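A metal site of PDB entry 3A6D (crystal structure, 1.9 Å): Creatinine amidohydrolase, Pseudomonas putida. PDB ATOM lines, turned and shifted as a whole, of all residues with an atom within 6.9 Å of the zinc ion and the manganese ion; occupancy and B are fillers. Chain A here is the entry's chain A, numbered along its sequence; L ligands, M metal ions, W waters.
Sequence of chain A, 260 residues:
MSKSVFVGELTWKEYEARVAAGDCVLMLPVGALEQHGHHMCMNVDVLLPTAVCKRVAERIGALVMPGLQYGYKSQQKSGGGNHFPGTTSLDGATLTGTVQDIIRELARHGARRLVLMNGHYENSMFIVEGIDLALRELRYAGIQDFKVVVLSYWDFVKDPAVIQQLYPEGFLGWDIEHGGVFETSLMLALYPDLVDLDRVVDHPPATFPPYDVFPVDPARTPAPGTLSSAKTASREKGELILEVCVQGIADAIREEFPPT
O of Ser 78 sits at hydrogen-bond distance from N3 of the ligand, 2.7 Å away.
OE1 of Glu 34 is in hydrogen-bond range of OG of Ser 74 (2.7 Å). A ring nitrogen (NE2) of His 120 sits close to the side-chain carboxylate of Glu 122, 3.4 Å away. A ring nitrogen (NE2) of His 178 is in hydrogen-bond range of the backbone carbonyl oxygen of Gln 35, 2.9 Å away. The backbone carbonyl oxygen of Glu 34 lies within hydrogen-bond range of a ring nitrogen (ND1) of His 36, at 2.7 Å. N of Gly 179 is in hydrogen-bond range of OE2 of Glu 183 (2.9 Å). NE2 of His 178 lies within hydrogen-bond range of O of Gly 79 (3.3 Å).
ND1 of His 178 touches the zinc ion, at 3.8 Å. Within 4 Å of the zinc ion: His 36, Asp 45, His 178 and Glu 183. The nearest printed residue that does not touch the zinc ion is Val 44 (4.2 Å).
Within 4 Å of the manganese ion: Glu 34, Asp 45 and His 120. Along chain A the residues within 4 Å of the manganese ion span positions 34 to 120. The nearest printed residue that does not touch the manganese ion is His 178 (4.1 Å).
The zinc ion is bound by the side-chain carboxylate of Glu 183 (2.1 Å), the side-chain carboxylate of Asp 45 (2.1 Å), water W2 (2.1 Å) and a ring nitrogen (NE2) of His 36 (2.2 Å). The zinc ion has four donor atoms within binding distance. Slightly farther from the zinc ion lies OE2 of Glu 183 (2.8 Å).
OE2 of Glu 34 binds the manganese ion (2.1 Å). The manganese ion is bound by OD2 of Asp 45 (2.1 Å). The manganese ion is bound by water W2. The manganese ion is bound by water W1 (2.3 Å). ND1 of His 120 binds the manganese ion, at 2.3 Å.
Water W2 lies within hydrogen-bond range of ND1 of His 178 (2.6 Å) and N3 of the ligand (2.9 Å). Water W1 lies within hydrogen-bond range of OE1 of Glu 122 (2.8 Å), OE1 of Glu 34 (2.9 Å) and N3 of the ligand (3.0 Å). Water W3 lies within hydrogen-bond range of N1 of the ligand, O of Gly 119 and N of Tyr 121.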
ATOM      1  N   GLY A  31      23.740 -21.906  -5.114  1.00  0.00           N
ATOM      2  CA  GLY A  31      22.826 -21.028  -5.810  1.00  0.00           C
ATOM      3  C   GLY A  31      21.909 -20.162  -4.972  1.00  0.00           C
ATOM      4  O   GLY A  31      22.329 -19.548  -3.989  1.00  0.00           O
ATOM      5  N   ALA A  32      20.639 -20.107  -5.391  1.00  0.00           N
ATOM      6  CA  ALA A  32      19.619 -19.309  -4.728  1.00  0.00           C
ATOM      7  C   ALA A  32      18.272 -19.481  -5.402  1.00  0.00           C
ATOM      8  O   ALA A  32      18.195 -20.001  -6.517  1.00  0.00           O
ATOM      9  CB  ALA A  32      20.006 -17.826  -4.747  1.00  0.00           C
ATOM     10  N   GLU A  34      15.557 -17.040  -6.535  1.00  0.00           N
ATOM     11  CA  GLU A  34      15.426 -15.597  -6.703  1.00  0.00           C
ATOM     12  C   GLU A  34      14.686 -15.208  -7.979  1.00  0.00           C
ATOM     13  O   GLU A  34      14.813 -15.869  -9.011  1.00  0.00           O
ATOM     14  CB  GLU A  34      16.849 -15.013  -6.726  1.00  0.00           C
ATOM     15  CG  GLU A  34      16.989 -13.504  -6.833  1.00  0.00           C
ATOM     16  CD  GLU A  34      18.428 -13.117  -7.147  1.00  0.00           C
ATOM     17  OE1 GLU A  34      18.888 -12.051  -6.698  1.00  0.00           O
ATOM     18  OE2 GLU A  34      19.098 -13.898  -7.854  1.00  0.00           O
ATOM     19  N   GLN A  35      13.927 -14.115  -7.916  1.00  0.00           N
ATOM     20  CA  GLN A  35      13.190 -13.641  -9.077  1.00  0.00           C
ATOM     21  C   GLN A  35      14.177 -13.390 -10.216  1.00  0.00           C
ATOM     22  O   GLN A  35      15.298 -12.940  -9.985  1.00  0.00           O
ATOM     23  CB  GLN A  35      12.430 -12.357  -8.735  1.00  0.00           C
ATOM     24  CG  GLN A  35      13.294 -11.132  -8.394  1.00  0.00           C
ATOM     25  CD  GLN A  35      13.842 -10.418  -9.622  1.00  0.00           C
ATOM     26  OE1 GLN A  35      13.266 -10.502 -10.709  1.00  0.00           O
ATOM     27  NE2 GLN A  35      14.944  -9.691  -9.452  1.00  0.00           N
ATOM     28  N   HIS A  36      13.745 -13.698 -11.434  1.00  0.00           N
ATOM     29  CA  HIS A  36      14.570 -13.484 -12.628  1.00  0.00           C
ATOM     30  C   HIS A  36      13.748 -12.892 -13.765  1.00  0.00           C
ATOM     31  O   HIS A  36      13.822 -13.376 -14.895  1.00  0.00           O
ATOM     32  CB  HIS A  36      15.206 -14.790 -13.093  1.00  0.00           C
ATOM     33  CG  HIS A  36      16.474 -15.136 -12.377  1.00  0.00           C
ATOM     34  ND1 HIS A  36      16.481 -15.607 -11.081  1.00  0.00           N
ATOM     35  CD2 HIS A  36      17.763 -15.040 -12.748  1.00  0.00           C
ATOM     36  CE1 HIS A  36      17.730 -15.788 -10.682  1.00  0.00           C
ATOM     37  NE2 HIS A  36      18.526 -15.449 -11.685  1.00  0.00           N
ATOM     38  N   MET A  40      11.829 -15.684 -17.073  1.00  0.00           N
ATOM     39  CA  MET A  40      12.532 -16.871 -16.582  1.00  0.00           C
ATOM     40  C   MET A  40      12.070 -17.318 -15.205  1.00  0.00           C
ATOM     41  O   MET A  40      11.495 -16.533 -14.460  1.00  0.00           O
ATOM     42  CB  MET A  40      14.045 -16.619 -16.502  1.00  0.00           C
ATOM     43  CG  MET A  40      14.773 -16.573 -17.814  1.00  0.00           C
ATOM     44  SD  MET A  40      16.506 -16.944 -17.552  1.00  0.00           S
ATOM     45  CE  MET A  40      17.065 -15.439 -16.753  1.00  0.00           C
ATOM     46  N   VAL A  44      17.200 -20.472 -11.447  1.00  0.00           N
ATOM     47  CA  VAL A  44      18.323 -20.280 -12.374  1.00  0.00           C
ATOM     48  C   VAL A  44      19.692 -20.422 -11.720  1.00  0.00           C
ATOM     49  O   VAL A  44      20.568 -21.135 -12.219  1.00  0.00           O
ATOM     50  CB  VAL A  44      18.234 -18.881 -13.043  1.00  0.00           C
ATOM     51  CG1 VAL A  44      19.490 -18.601 -13.840  1.00  0.00           C
ATOM     52  CG2 VAL A  44      17.004 -18.814 -13.950  1.00  0.00           C
ATOM     53  N   ASP A  45      19.891 -19.745 -10.592  1.00  0.00           N
ATOM     54  CA  ASP A  45      21.190 -19.775  -9.908  1.00  0.00           C
ATOM     55  C   ASP A  45      21.623 -21.129  -9.392  1.00  0.00           C
ATOM     56  O   ASP A  45      22.790 -21.303  -9.040  1.00  0.00           O
ATOM     57  CB  ASP A  45      21.212 -18.734  -8.787  1.00  0.00           C
ATOM     58  CG  ASP A  45      21.178 -17.327  -9.330  1.00  0.00           C
ATOM     59  OD1 ASP A  45      21.181 -17.198 -10.572  1.00  0.00           O
ATOM     60  OD2 ASP A  45      21.156 -16.372  -8.545  1.00  0.00           O
ATOM     61  N   LEU A  48      22.087 -23.427 -13.363  1.00  0.00           N
ATOM     62  CA  LEU A  48      23.269 -23.136 -14.160  1.00  0.00           C
ATOM     63  C   LEU A  48      24.597 -23.648 -13.582  1.00  0.00           C
ATOM     64  O   LEU A  48      25.324 -24.349 -14.279  1.00  0.00           O
ATOM     65  CB  LEU A  48      23.337 -21.633 -14.457  1.00  0.00           C
ATOM     66  CG  LEU A  48      22.095 -21.129 -15.223  1.00  0.00           C
ATOM     67  CD1 LEU A  48      22.289 -19.674 -15.643  1.00  0.00           C
ATOM     68  CD2 LEU A  48      21.855 -21.990 -16.456  1.00  0.00           C
ATOM     69  N   SER A  74      19.156 -11.044  -1.887  1.00  0.00           N
ATOM     70  CA  SER A  74      19.357 -10.367  -3.155  1.00  0.00           C
ATOM     71  C   SER A  74      19.621  -8.885  -2.886  1.00  0.00           C
ATOM     72  O   SER A  74      18.938  -8.271  -2.070  1.00  0.00           O
ATOM     73  CB  SER A  74      18.091 -10.524  -4.020  1.00  0.00           C
ATOM     74  OG  SER A  74      18.244  -9.898  -5.285  1.00  0.00           O
ATOM     75  N   SER A  78      22.736  -5.792  -7.761  1.00  0.00           N
ATOM     76  CA  SER A  78      23.209  -7.002  -8.408  1.00  0.00           C
ATOM     77  C   SER A  78      22.134  -8.051  -8.679  1.00  0.00           C
ATOM     78  O   SER A  78      22.328  -8.937  -9.507  1.00  0.00           O
ATOM     79  CB  SER A  78      24.340  -7.632  -7.586  1.00  0.00           C
ATOM     80  OG  SER A  78      23.966  -7.786  -6.222  1.00  0.00           O
ATOM     81  N   GLY A  79      21.011  -7.954  -7.979  1.00  0.00           N
ATOM     82  CA  GLY A  79      19.948  -8.934  -8.168  1.00  0.00           C
ATOM     83  C   GLY A  79      18.536  -8.385  -8.096  1.00  0.00           C
ATOM     84  O   GLY A  79      17.585  -9.160  -8.004  1.00  0.00           O
ATOM     85  N   GLY A 119      26.772 -19.490  -8.057  1.00  0.00           N
ATOM     86  CA  GLY A 119      25.945 -19.098  -9.180  1.00  0.00           C
ATOM     87  C   GLY A 119      25.083 -17.886  -8.842  1.00  0.00           C
ATOM     88  O   GLY A 119      24.343 -17.389  -9.691  1.00  0.00           O
ATOM     89  N   HIS A 120      25.190 -17.416  -7.597  1.00  0.00           N
ATOM     90  CA  HIS A 120      24.417 -16.264  -7.111  1.00  0.00           C
ATOM     91  C   HIS A 120      25.408 -15.209  -6.611  1.00  0.00           C
ATOM     92  O   HIS A 120      26.066 -15.384  -5.590  1.00  0.00           O
ATOM     93  CB  HIS A 120      23.477 -16.720  -5.976  1.00  0.00           C
ATOM     94  CG  HIS A 120      22.685 -15.613  -5.342  1.00  0.00           C
ATOM     95  ND1 HIS A 120      21.833 -14.798  -6.058  1.00  0.00           N
ATOM     96  CD2 HIS A 120      22.565 -15.230  -4.045  1.00  0.00           C
ATOM     97  CE1 HIS A 120      21.222 -13.957  -5.234  1.00  0.00           C
ATOM     98  NE2 HIS A 120      21.651 -14.201  -4.010  1.00  0.00           N
ATOM     99  N   TYR A 121      25.505 -14.124  -7.369  1.00  0.00           N
ATOM    100  CA  TYR A 121      26.432 -13.024  -7.098  1.00  0.00           C
ATOM    101  C   TYR A 121      26.647 -12.681  -5.618  1.00  0.00           C
ATOM    102  O   TYR A 121      27.784 -12.600  -5.160  1.00  0.00           O
ATOM    103  CB  TYR A 121      25.937 -11.775  -7.836  1.00  0.00           C
ATOM    104  CG  TYR A 121      26.960 -10.663  -7.936  1.00  0.00           C
ATOM    105  CD1 TYR A 121      27.741 -10.509  -9.079  1.00  0.00           C
ATOM    106  CD2 TYR A 121      27.125  -9.754  -6.896  1.00  0.00           C
ATOM    107  CE1 TYR A 121      28.661  -9.461  -9.191  1.00  0.00           C
ATOM    108  CE2 TYR A 121      28.045  -8.703  -6.990  1.00  0.00           C
ATOM    109  CZ  TYR A 121      28.809  -8.575  -8.141  1.00  0.00           C
ATOM    110  OH  TYR A 121      29.709  -7.533  -8.239  1.00  0.00           O
ATOM    111  N   GLU A 122      25.555 -12.513  -4.883  1.00  0.00           N
ATOM    112  CA  GLU A 122      25.601 -12.139  -3.475  1.00  0.00           C
ATOM    113  C   GLU A 122      26.160 -13.161  -2.464  1.00  0.00           C
ATOM    114  O   GLU A 122      26.485 -12.771  -1.339  1.00  0.00           O
ATOM    115  CB  GLU A 122      24.206 -11.699  -3.012  1.00  0.00           C
ATOM    116  CG  GLU A 122      23.699 -10.412  -3.680  1.00  0.00           C
ATOM    117  CD  GLU A 122      22.997 -10.651  -5.010  1.00  0.00           C
ATOM    118  OE1 GLU A 122      23.280 -11.664  -5.685  1.00  0.00           O
ATOM    119  OE2 GLU A 122      22.169  -9.806  -5.398  1.00  0.00           O
ATOM    120  N   TYR A 153      31.159 -18.903 -11.793  1.00  0.00           N
ATOM    121  CA  TYR A 153      31.381 -19.349 -13.164  1.00  0.00           C
ATOM    122  C   TYR A 153      31.462 -18.311 -14.283  1.00  0.00           C
ATOM    123  O   TYR A 153      32.242 -18.478 -15.217  1.00  0.00           O
ATOM    124  CB  TYR A 153      30.373 -20.463 -13.503  1.00  0.00           C
ATOM    125  CG  TYR A 153      28.969 -20.002 -13.767  1.00  0.00           C
ATOM    126  CD1 TYR A 153      28.536 -19.716 -15.062  1.00  0.00           C
ATOM    127  CD2 TYR A 153      28.058 -19.839 -12.719  1.00  0.00           C
ATOM    128  CE1 TYR A 153      27.250 -19.272 -15.314  1.00  0.00           C
ATOM    129  CE2 TYR A 153      26.753 -19.401 -12.958  1.00  0.00           C
ATOM    130  CZ  TYR A 153      26.363 -19.116 -14.265  1.00  0.00           C
ATOM    131  OH  TYR A 153      25.096 -18.656 -14.520  1.00  0.00           O
ATOM    132  N   TRP A 154      30.690 -17.225 -14.196  1.00  0.00           N
ATOM    133  CA  TRP A 154      30.737 -16.217 -15.250  1.00  0.00           C
ATOM    134  C   TRP A 154      32.088 -15.511 -15.380  1.00  0.00           C
ATOM    135  O   TRP A 154      32.400 -14.952 -16.432  1.00  0.00           O
ATOM    136  CB  TRP A 154      29.626 -15.177 -15.056  1.00  0.00           C
ATOM    137  CG  TRP A 154      29.627 -14.538 -13.701  1.00  0.00           C
ATOM    138  CD1 TRP A 154      30.443 -13.531 -13.267  1.00  0.00           C
ATOM    139  CD2 TRP A 154      28.769 -14.870 -12.605  1.00  0.00           C
ATOM    140  NE1 TRP A 154      30.146 -13.226 -11.948  1.00  0.00           N
ATOM    141  CE2 TRP A 154      29.130 -14.030 -11.522  1.00  0.00           C
ATOM    142  CE3 TRP A 154      27.738 -15.808 -12.427  1.00  0.00           C
ATOM    143  CZ2 TRP A 154      28.488 -14.095 -10.279  1.00  0.00           C
ATOM    144  CZ3 TRP A 154      27.096 -15.873 -11.184  1.00  0.00           C
ATOM    145  CH2 TRP A 154      27.481 -15.016 -10.133  1.00  0.00           C
ATOM    146  N   GLU A 177      24.169  -8.083 -14.802  1.00  0.00           N
ATOM    147  CA  GLU A 177      23.880  -9.265 -15.598  1.00  0.00           C
ATOM    148  C   GLU A 177      22.943 -10.203 -14.808  1.00  0.00           C
ATOM    149  O   GLU A 177      23.227 -11.389 -14.648  1.00  0.00           O
ATOM    150  CB  GLU A 177      25.192  -9.962 -15.955  1.00  0.00           C
ATOM    151  CG  GLU A 177      25.122 -10.852 -17.187  1.00  0.00           C
ATOM    152  CD  GLU A 177      24.394 -10.191 -18.348  1.00  0.00           C
ATOM    153  OE1 GLU A 177      24.909  -9.215 -18.927  1.00  0.00           O
ATOM    154  OE2 GLU A 177      23.279 -10.658 -18.670  1.00  0.00           O
ATOM    155  N   HIS A 178      21.852  -9.643 -14.310  1.00  0.00           N
ATOM    156  CA  HIS A 178      20.863 -10.436 -13.577  1.00  0.00           C
ATOM    157  C   HIS A 178      19.621 -10.563 -14.447  1.00  0.00           C
ATOM    158  O   HIS A 178      18.918  -9.576 -14.678  1.00  0.00           O
ATOM    159  CB  HIS A 178      20.483  -9.776 -12.254  1.00  0.00           C
ATOM    160  CG  HIS A 178      19.378 -10.492 -11.531  1.00  0.00           C
ATOM    161  ND1 HIS A 178      19.536 -11.756 -11.001  1.00  0.00           N
ATOM    162  CD2 HIS A 178      18.083 -10.142 -11.312  1.00  0.00           C
ATOM    163  CE1 HIS A 178      18.382 -12.155 -10.479  1.00  0.00           C
ATOM    164  NE2 HIS A 178      17.492 -11.193 -10.662  1.00  0.00           N
ATOM    165  N   GLY A 179      19.361 -11.778 -14.923  1.00  0.00           N
ATOM    166  CA  GLY A 179      18.193 -11.987 -15.764  1.00  0.00           C
ATOM    167  C   GLY A 179      18.376 -11.359 -17.135  1.00  0.00           C
ATOM    168  O   GLY A 179      17.410 -11.116 -17.840  1.00  0.00           O
ATOM    169  N   GLU A 183      22.646 -15.046 -18.445  1.00  0.00           N
ATOM    170  CA  GLU A 183      21.881 -16.146 -17.860  1.00  0.00           C
ATOM    171  C   GLU A 183      20.778 -16.639 -18.774  1.00  0.00           C
ATOM    172  O   GLU A 183      20.569 -17.846 -18.907  1.00  0.00           O
ATOM    173  CB  GLU A 183      21.259 -15.724 -16.518  1.00  0.00           C
ATOM    174  CG  GLU A 183      22.266 -15.405 -15.441  1.00  0.00           C
ATOM    175  CD  GLU A 183      21.596 -15.114 -14.119  1.00  0.00           C
ATOM    176  OE1 GLU A 183      21.908 -15.827 -13.140  1.00  0.00           O
ATOM    177  OE2 GLU A 183      20.759 -14.184 -14.058  1.00  0.00           O
HETATM  178  C1  LIG L   1      25.915 -12.242 -12.433  1.00  0.00           C
HETATM  179  N1  LIG L   1      24.851 -12.313 -11.614  1.00  0.00           N
HETATM  180  C2  LIG L   1      24.199 -11.227 -11.137  1.00  0.00           C
HETATM  181  N2  LIG L   1      24.560  -9.976 -11.428  1.00  0.00           N
HETATM  182  N3  LIG L   1      23.157 -11.422 -10.333  1.00  0.00           N
HETATM  183 ZN    ZN M   1      20.676 -15.341 -11.500  1.00  0.00          ZN
HETATM  184 MN    MN M   2      21.151 -14.259  -8.236  1.00  0.00          MN
HETATM  185  O   HOH W   1      21.496 -12.039  -7.874  1.00  0.00           O
HETATM  186  O   HOH W   2      21.274 -13.623 -10.379  1.00  0.00           O
HETATM  187  O   HOH W   3      23.734 -14.420 -10.016  1.00  0.00           O
